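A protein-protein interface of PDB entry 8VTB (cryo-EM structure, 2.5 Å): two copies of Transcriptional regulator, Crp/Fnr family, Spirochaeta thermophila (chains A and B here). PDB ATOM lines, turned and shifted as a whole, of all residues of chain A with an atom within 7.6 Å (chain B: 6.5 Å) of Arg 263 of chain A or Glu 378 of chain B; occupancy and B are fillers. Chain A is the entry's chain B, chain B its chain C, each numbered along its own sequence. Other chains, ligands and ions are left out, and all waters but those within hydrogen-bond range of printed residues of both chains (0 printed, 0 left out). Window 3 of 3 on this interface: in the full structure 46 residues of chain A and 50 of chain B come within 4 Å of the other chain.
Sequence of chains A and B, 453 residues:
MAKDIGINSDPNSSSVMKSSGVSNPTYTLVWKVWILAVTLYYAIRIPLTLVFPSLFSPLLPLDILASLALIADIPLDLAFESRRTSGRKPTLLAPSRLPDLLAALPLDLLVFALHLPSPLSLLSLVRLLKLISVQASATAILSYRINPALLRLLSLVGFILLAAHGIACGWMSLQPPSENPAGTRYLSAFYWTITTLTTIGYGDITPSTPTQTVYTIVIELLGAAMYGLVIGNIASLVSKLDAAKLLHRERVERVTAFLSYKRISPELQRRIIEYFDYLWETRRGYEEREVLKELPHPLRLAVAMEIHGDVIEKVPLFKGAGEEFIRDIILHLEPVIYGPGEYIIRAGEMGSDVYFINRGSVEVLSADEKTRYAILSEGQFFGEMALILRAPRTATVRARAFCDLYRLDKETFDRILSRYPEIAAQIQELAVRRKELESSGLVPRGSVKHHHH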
ATOM      1  N   ALA A 257      21.021  22.775  -8.795  1.00  0.00           N
ATOM      2  CA  ALA A 257      20.858  23.349 -10.125  1.00  0.00           C
ATOM      3  C   ALA A 257      19.387  23.433 -10.506  1.00  0.00           C
ATOM      4  O   ALA A 257      18.923  24.459 -11.023  1.00  0.00           O
ATOM      5  CB  ALA A 257      21.640  22.527 -11.150  1.00  0.00           C
ATOM      6  N   PHE A 258      18.629  22.363 -10.251  1.00  0.00           N
ATOM      7  CA  PHE A 258      17.210  22.396 -10.590  1.00  0.00           C
ATOM      8  C   PHE A 258      16.474  23.471  -9.800  1.00  0.00           C
ATOM      9  O   PHE A 258      15.635  24.190 -10.353  1.00  0.00           O
ATOM     10  CB  PHE A 258      16.571  21.032 -10.360  1.00  0.00           C
ATOM     11  CG  PHE A 258      15.160  20.957 -10.841  1.00  0.00           C
ATOM     12  CD1 PHE A 258      14.885  20.721 -12.177  1.00  0.00           C
ATOM     13  CD2 PHE A 258      14.108  21.145  -9.963  1.00  0.00           C
ATOM     14  CE1 PHE A 258      13.588  20.665 -12.623  1.00  0.00           C
ATOM     15  CE2 PHE A 258      12.809  21.088 -10.407  1.00  0.00           C
ATOM     16  CZ  PHE A 258      12.552  20.853 -11.738  1.00  0.00           C
ATOM     17  N   LEU A 259      16.767  23.592  -8.505  1.00  0.00           N
ATOM     18  CA  LEU A 259      16.115  24.620  -7.702  1.00  0.00           C
ATOM     19  C   LEU A 259      16.528  26.016  -8.143  1.00  0.00           C
ATOM     20  O   LEU A 259      15.734  26.957  -8.041  1.00  0.00           O
ATOM     21  CB  LEU A 259      16.432  24.411  -6.224  1.00  0.00           C
ATOM     22  CG  LEU A 259      15.902  23.119  -5.602  1.00  0.00           C
ATOM     23  CD1 LEU A 259      16.487  22.924  -4.219  1.00  0.00           C
ATOM     24  CD2 LEU A 259      14.385  23.113  -5.553  1.00  0.00           C
ATOM     25  N   SER A 260      17.762  26.172  -8.628  1.00  0.00           N
ATOM     26  CA  SER A 260      18.187  27.450  -9.180  1.00  0.00           C
ATOM     27  C   SER A 260      17.398  27.788 -10.437  1.00  0.00           C
ATOM     28  O   SER A 260      17.035  28.950 -10.655  1.00  0.00           O
ATOM     29  CB  SER A 260      19.686  27.427  -9.474  1.00  0.00           C
ATOM     30  OG  SER A 260      19.951  26.807 -10.719  1.00  0.00           O
ATOM     31  N   TYR A 261      17.132  26.787 -11.281  1.00  0.00           N
ATOM     32  CA  TYR A 261      16.285  27.023 -12.448  1.00  0.00           C
ATOM     33  C   TYR A 261      14.884  27.462 -12.037  1.00  0.00           C
ATOM     34  O   TYR A 261      14.313  28.382 -12.634  1.00  0.00           O
ATOM     35  CB  TYR A 261      16.215  25.773 -13.322  1.00  0.00           C
ATOM     36  CG  TYR A 261      15.140  25.852 -14.381  1.00  0.00           C
ATOM     37  CD1 TYR A 261      15.284  26.682 -15.485  1.00  0.00           C
ATOM     38  CD2 TYR A 261      13.972  25.110 -14.267  1.00  0.00           C
ATOM     39  CE1 TYR A 261      14.300  26.764 -16.449  1.00  0.00           C
ATOM     40  CE2 TYR A 261      12.982  25.186 -15.226  1.00  0.00           C
ATOM     41  CZ  TYR A 261      13.154  26.013 -16.313  1.00  0.00           C
ATOM     42  OH  TYR A 261      12.172  26.094 -17.273  1.00  0.00           O
ATOM     43  N   LYS A 262      14.311  26.815 -11.019  1.00  0.00           N
ATOM     44  CA  LYS A 262      12.980  27.161 -10.528  1.00  0.00           C
ATOM     45  C   LYS A 262      12.946  28.452  -9.723  1.00  0.00           C
ATOM     46  O   LYS A 262      11.880  28.794  -9.200  1.00  0.00           O
ATOM     47  CB  LYS A 262      12.417  26.016  -9.685  1.00  0.00           C
ATOM     48  CG  LYS A 262      12.110  24.756 -10.470  1.00  0.00           C
ATOM     49  CD  LYS A 262      11.009  25.016 -11.484  1.00  0.00           C
ATOM     50  CE  LYS A 262      10.614  23.744 -12.210  1.00  0.00           C
ATOM     51  NZ  LYS A 262       9.453  23.958 -13.116  1.00  0.00           N
ATOM     52  N   ARG A 263      14.067  29.168  -9.608  1.00  0.00           N
ATOM     53  CA  ARG A 263      14.122  30.452  -8.905  1.00  0.00           C
ATOM     54  C   ARG A 263      13.702  30.319  -7.444  1.00  0.00           C
ATOM     55  O   ARG A 263      13.043  31.202  -6.893  1.00  0.00           O
ATOM     56  CB  ARG A 263      13.274  31.507  -9.621  1.00  0.00           C
ATOM     57  CG  ARG A 263      13.598  31.638 -11.102  1.00  0.00           C
ATOM     58  CD  ARG A 263      12.729  32.676 -11.789  1.00  0.00           C
ATOM     59  NE  ARG A 263      11.309  32.373 -11.662  1.00  0.00           N
ATOM     60  CZ  ARG A 263      10.392  32.704 -12.560  1.00  0.00           C
ATOM     61  NH1 ARG A 263      10.712  33.354 -13.666  1.00  0.00           N
ATOM     62  NH2 ARG A 263       9.122  32.367 -12.345  1.00  0.00           N
ATOM     63  N   ILE A 264      14.076  29.205  -6.815  1.00  0.00           N
ATOM     64  CA  ILE A 264      13.807  29.007  -5.397  1.00  0.00           C
ATOM     65  C   ILE A 264      14.607  30.010  -4.580  1.00  0.00           C
ATOM     66  O   ILE A 264      15.758  30.333  -4.908  1.00  0.00           O
ATOM     67  CB  ILE A 264      14.133  27.558  -4.997  1.00  0.00           C
ATOM     68  CG1 ILE A 264      13.233  26.584  -5.760  1.00  0.00           C
ATOM     69  CG2 ILE A 264      13.989  27.355  -3.500  1.00  0.00           C
ATOM     70  CD1 ILE A 264      11.768  26.719  -5.416  1.00  0.00           C
ATOM     71  N   SER A 265      13.994  30.523  -3.513  1.00  0.00           N
ATOM     72  CA  SER A 265      14.652  31.514  -2.677  1.00  0.00           C
ATOM     73  C   SER A 265      15.853  30.895  -1.960  1.00  0.00           C
ATOM     74  O   SER A 265      15.846  29.705  -1.633  1.00  0.00           O
ATOM     75  CB  SER A 265      13.671  32.089  -1.658  1.00  0.00           C
ATOM     76  OG  SER A 265      13.188  31.078  -0.792  1.00  0.00           O
ATOM     77  N   PRO A 266      16.902  31.685  -1.707  1.00  0.00           N
ATOM     78  CA  PRO A 266      18.103  31.123  -1.068  1.00  0.00           C
ATOM     79  C   PRO A 266      17.898  30.597   0.346  1.00  0.00           C
ATOM     80  O   PRO A 266      18.696  29.762   0.787  1.00  0.00           O
ATOM     81  CB  PRO A 266      19.095  32.295  -1.106  1.00  0.00           C
ATOM     82  CG  PRO A 266      18.258  33.516  -1.187  1.00  0.00           C
ATOM     83  CD  PRO A 266      17.040  33.125  -1.985  1.00  0.00           C
ATOM     84  N   GLN A 269      16.787  27.053  -0.178  1.00  0.00           N
ATOM     85  CA  GLN A 269      17.953  26.341  -0.690  1.00  0.00           C
ATOM     86  C   GLN A 269      18.943  26.036   0.427  1.00  0.00           C
ATOM     87  O   GLN A 269      19.526  24.949   0.467  1.00  0.00           O
ATOM     88  CB  GLN A 269      18.617  27.155  -1.799  1.00  0.00           C
ATOM     89  CG  GLN A 269      17.776  27.269  -3.059  1.00  0.00           C
ATOM     90  CD  GLN A 269      18.611  27.512  -4.300  1.00  0.00           C
ATOM     91  OE1 GLN A 269      18.621  28.612  -4.851  1.00  0.00           O
ATOM     92  NE2 GLN A 269      19.316  26.480  -4.749  1.00  0.00           N
ATOM     93  N   GLU B 306       6.655  26.899  -2.940  1.00  0.00           N
ATOM     94  CA  GLU B 306       7.434  28.025  -3.443  1.00  0.00           C
ATOM     95  C   GLU B 306       7.225  28.212  -4.940  1.00  0.00           C
ATOM     96  O   GLU B 306       7.001  29.334  -5.411  1.00  0.00           O
ATOM     97  CB  GLU B 306       8.912  27.804  -3.132  1.00  0.00           C
ATOM     98  CG  GLU B 306       9.797  28.998  -3.409  1.00  0.00           C
ATOM     99  CD  GLU B 306      10.132  29.764  -2.149  1.00  0.00           C
ATOM    100  OE1 GLU B 306       9.204  30.061  -1.367  1.00  0.00           O
ATOM    101  OE2 GLU B 306      11.323  30.058  -1.936  1.00  0.00           O
ATOM    102  N   VAL B 311      -0.331  30.899  -7.508  1.00  0.00           N
ATOM    103  CA  VAL B 311      -0.945  30.515  -8.778  1.00  0.00           C
ATOM    104  C   VAL B 311      -2.178  29.653  -8.547  1.00  0.00           C
ATOM    105  O   VAL B 311      -3.164  29.751  -9.288  1.00  0.00           O
ATOM    106  CB  VAL B 311       0.090  29.801  -9.666  1.00  0.00           C
ATOM    107  CG1 VAL B 311      -0.562  29.250 -10.924  1.00  0.00           C
ATOM    108  CG2 VAL B 311       1.229  30.744 -10.012  1.00  0.00           C
ATOM    109  N   ILE B 357       0.421  27.628 -16.032  1.00  0.00           N
ATOM    110  CA  ILE B 357       1.590  28.036 -16.801  1.00  0.00           C
ATOM    111  C   ILE B 357       2.674  28.468 -15.822  1.00  0.00           C
ATOM    112  O   ILE B 357       2.553  29.509 -15.169  1.00  0.00           O
ATOM    113  CB  ILE B 357       1.254  29.162 -17.785  1.00  0.00           C
ATOM    114  CG1 ILE B 357       0.079  28.766 -18.678  1.00  0.00           C
ATOM    115  CG2 ILE B 357       2.466  29.503 -18.633  1.00  0.00           C
ATOM    116  CD1 ILE B 357      -0.556  29.928 -19.396  1.00  0.00           C
ATOM    117  N   ASN B 358       3.736  27.673 -15.718  1.00  0.00           N
ATOM    118  CA  ASN B 358       4.880  28.055 -14.904  1.00  0.00           C
ATOM    119  C   ASN B 358       5.900  28.861 -15.691  1.00  0.00           C
ATOM    120  O   ASN B 358       6.534  29.763 -15.132  1.00  0.00           O
ATOM    121  CB  ASN B 358       5.553  26.812 -14.319  1.00  0.00           C
ATOM    122  CG  ASN B 358       6.752  27.148 -13.459  1.00  0.00           C
ATOM    123  OD1 ASN B 358       7.886  26.807 -13.794  1.00  0.00           O
ATOM    124  ND2 ASN B 358       6.509  27.816 -12.337  1.00  0.00           N
ATOM    125  N   ARG B 359       6.062  28.562 -16.978  1.00  0.00           N
ATOM    126  CA  ARG B 359       6.902  29.378 -17.843  1.00  0.00           C
ATOM    127  C   ARG B 359       6.451  29.198 -19.282  1.00  0.00           C
ATOM    128  O   ARG B 359       5.858  28.179 -19.642  1.00  0.00           O
ATOM    129  CB  ARG B 359       8.387  29.031 -17.695  1.00  0.00           C
ATOM    130  CG  ARG B 359       9.293  30.254 -17.689  1.00  0.00           C
ATOM    131  CD  ARG B 359      10.694  29.933 -17.198  1.00  0.00           C
ATOM    132  NE  ARG B 359      10.706  29.508 -15.803  1.00  0.00           N
ATOM    133  CZ  ARG B 359      11.804  29.358 -15.077  1.00  0.00           C
ATOM    134  NH1 ARG B 359      13.005  29.603 -15.578  1.00  0.00           N
ATOM    135  NH2 ARG B 359      11.696  28.954 -13.814  1.00  0.00           N
ATOM    136  N   GLY B 360       6.788  30.182 -20.111  1.00  0.00           N
ATOM    137  CA  GLY B 360       6.302  30.228 -21.473  1.00  0.00           C
ATOM    138  C   GLY B 360       4.921  30.848 -21.556  1.00  0.00           C
ATOM    139  O   GLY B 360       4.378  31.377 -20.580  1.00  0.00           O
ATOM    140  N   SER B 361       4.341  30.779 -22.752  1.00  0.00           N
ATOM    141  CA  SER B 361       3.034  31.375 -22.979  1.00  0.00           C
ATOM    142  C   SER B 361       2.271  30.553 -24.004  1.00  0.00           C
ATOM    143  O   SER B 361       2.856  29.897 -24.867  1.00  0.00           O
ATOM    144  CB  SER B 361       3.153  32.831 -23.447  1.00  0.00           C
ATOM    145  OG  SER B 361       3.961  32.928 -24.606  1.00  0.00           O
ATOM    146  N   LEU B 376      -2.176  33.778 -22.866  1.00  0.00           N
ATOM    147  CA  LEU B 376      -1.931  33.587 -21.444  1.00  0.00           C
ATOM    148  C   LEU B 376      -0.445  33.343 -21.225  1.00  0.00           C
ATOM    149  O   LEU B 376       0.214  32.703 -22.049  1.00  0.00           O
ATOM    150  CB  LEU B 376      -2.749  32.420 -20.893  1.00  0.00           C
ATOM    151  CG  LEU B 376      -4.256  32.470 -21.158  1.00  0.00           C
ATOM    152  CD1 LEU B 376      -4.934  31.210 -20.649  1.00  0.00           C
ATOM    153  CD2 LEU B 376      -4.868  33.709 -20.526  1.00  0.00           C
ATOM    154  N   SER B 377       0.084  33.860 -20.121  1.00  0.00           N
ATOM    155  CA  SER B 377       1.519  33.855 -19.883  1.00  0.00           C
ATOM    156  C   SER B 377       1.817  33.285 -18.502  1.00  0.00           C
ATOM    157  O   SER B 377       0.934  32.765 -17.812  1.00  0.00           O
ATOM    158  CB  SER B 377       2.109  35.265 -20.027  1.00  0.00           C
ATOM    159  OG  SER B 377       3.522  35.221 -20.108  1.00  0.00           O
ATOM    160  N   GLU B 378       3.089  33.373 -18.119  1.00  0.00           N
ATOM    161  CA  GLU B 378       3.598  32.868 -16.851  1.00  0.00           C
ATOM    162  C   GLU B 378       2.738  33.322 -15.680  1.00  0.00           C
ATOM    163  O   GLU B 378       2.458  34.513 -15.523  1.00  0.00           O
ATOM    164  CB  GLU B 378       5.041  33.342 -16.661  1.00  0.00           C
ATOM    165  CG  GLU B 378       5.664  32.954 -15.334  1.00  0.00           C
ATOM    166  CD  GLU B 378       7.130  33.334 -15.255  1.00  0.00           C
ATOM    167  OE1 GLU B 378       7.708  33.697 -16.301  1.00  0.00           O
ATOM    168  OE2 GLU B 378       7.705  33.269 -14.147  1.00  0.00           O
ATOM    169  N   GLY B 379       2.319  32.363 -14.859  1.00  0.00           N
ATOM    170  CA  GLY B 379       1.498  32.636 -13.701  1.00  0.00           C
ATOM    171  C   GLY B 379       0.004  32.556 -13.927  1.00  0.00           C
ATOM    172  O   GLY B 379      -0.758  32.732 -12.966  1.00  0.00           O
ATOM    173  N   GLN B 380      -0.445  32.298 -15.151  1.00  0.00           N
ATOM    174  CA  GLN B 380      -1.861  32.155 -15.447  1.00  0.00           C
ATOM    175  C   GLN B 380      -2.227  30.685 -15.622  1.00  0.00           C
ATOM    176  O   GLN B 380      -1.373  29.796 -15.612  1.00  0.00           O
ATOM    177  CB  GLN B 380      -2.236  32.960 -16.695  1.00  0.00           C
ATOM    178  CG  GLN B 380      -1.952  34.444 -16.567  1.00  0.00           C
ATOM    179  CD  GLN B 380      -2.343  35.219 -17.807  1.00  0.00           C
ATOM    180  OE1 GLN B 380      -1.544  35.381 -18.729  1.00  0.00           O
ATOM    181  NE2 GLN B 380      -3.580  35.700 -17.837  1.00  0.00           N
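NH2 of Arg 359 of chain B touches CA of Lys 262 of chain A, 3.96 Å away. Ile 264 of chain A touches Glu 306 of chain B (CD1 to CG, 3.6 Å).
The backbone NH (N) of Ile 264 of chain A sits at hydrogen-bond distance from the backbone carbonyl oxygen (O) of Leu 259 of chain A (3.1 Å). The backbone carbonyl oxygen (O) of Ile 264 of chain A sits close to the side-chain amide oxygen (OE1) of Gln 269 of chain A. N of Glu 378 of chain B is in hydrogen-bond range of O of Gly 360 of chain B (3.4 Å).
The backbone carbonyl oxygen of Tyr 261 of chain A is in hydrogen-bond range of the guanidinium group of Arg 359 of chain B, at 2.9 Å. NZ of Lys 262 of chain A is in hydrogen-bond range of OD1 of Asn 358 of chain B (3.3 Å). The guanidinium group (NH2) of Arg 263 of chain A is in salt-bridge range of the side-chain carboxylate (OE2) of Glu 378 of chain B. The side-chain carboxylate of Glu 306 of chain B sits at hydrogen-bond distance from the side-chain hydroxyl of Ser 265 of chain A (2.4 Å).
Of chain A, only Arg 263 comes within 4 Å of Glu 378 of chain B. Of the printed residues of chain B, Tyr 261 of chain A touches Arg 359 (2.9 Å). Of the printed residues of chain A, Asn 358 of chain B touches Lys 262 (3.3 Å). The nearest residue of chain B that does not touch Arg 263 of chain A is Arg 359 of chain B (4.1 Å). The nearest printed residue of chain B that does not touch Tyr 261 of chain A is Asn 358 of chain B (5.5 Å).
Of the 11 printed residues of chain A, 5 touch a printed residue of chain B. Hydrophobic or aromatic side chains of chain A that line the printed part of chain B: Tyr 261 and Ile 264. Of the 12 printed residues of chain B, 4 touch a printed residue of chain A. Among the printed residues, 6 pairs touch across the chains.
No position is printed for both chains.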
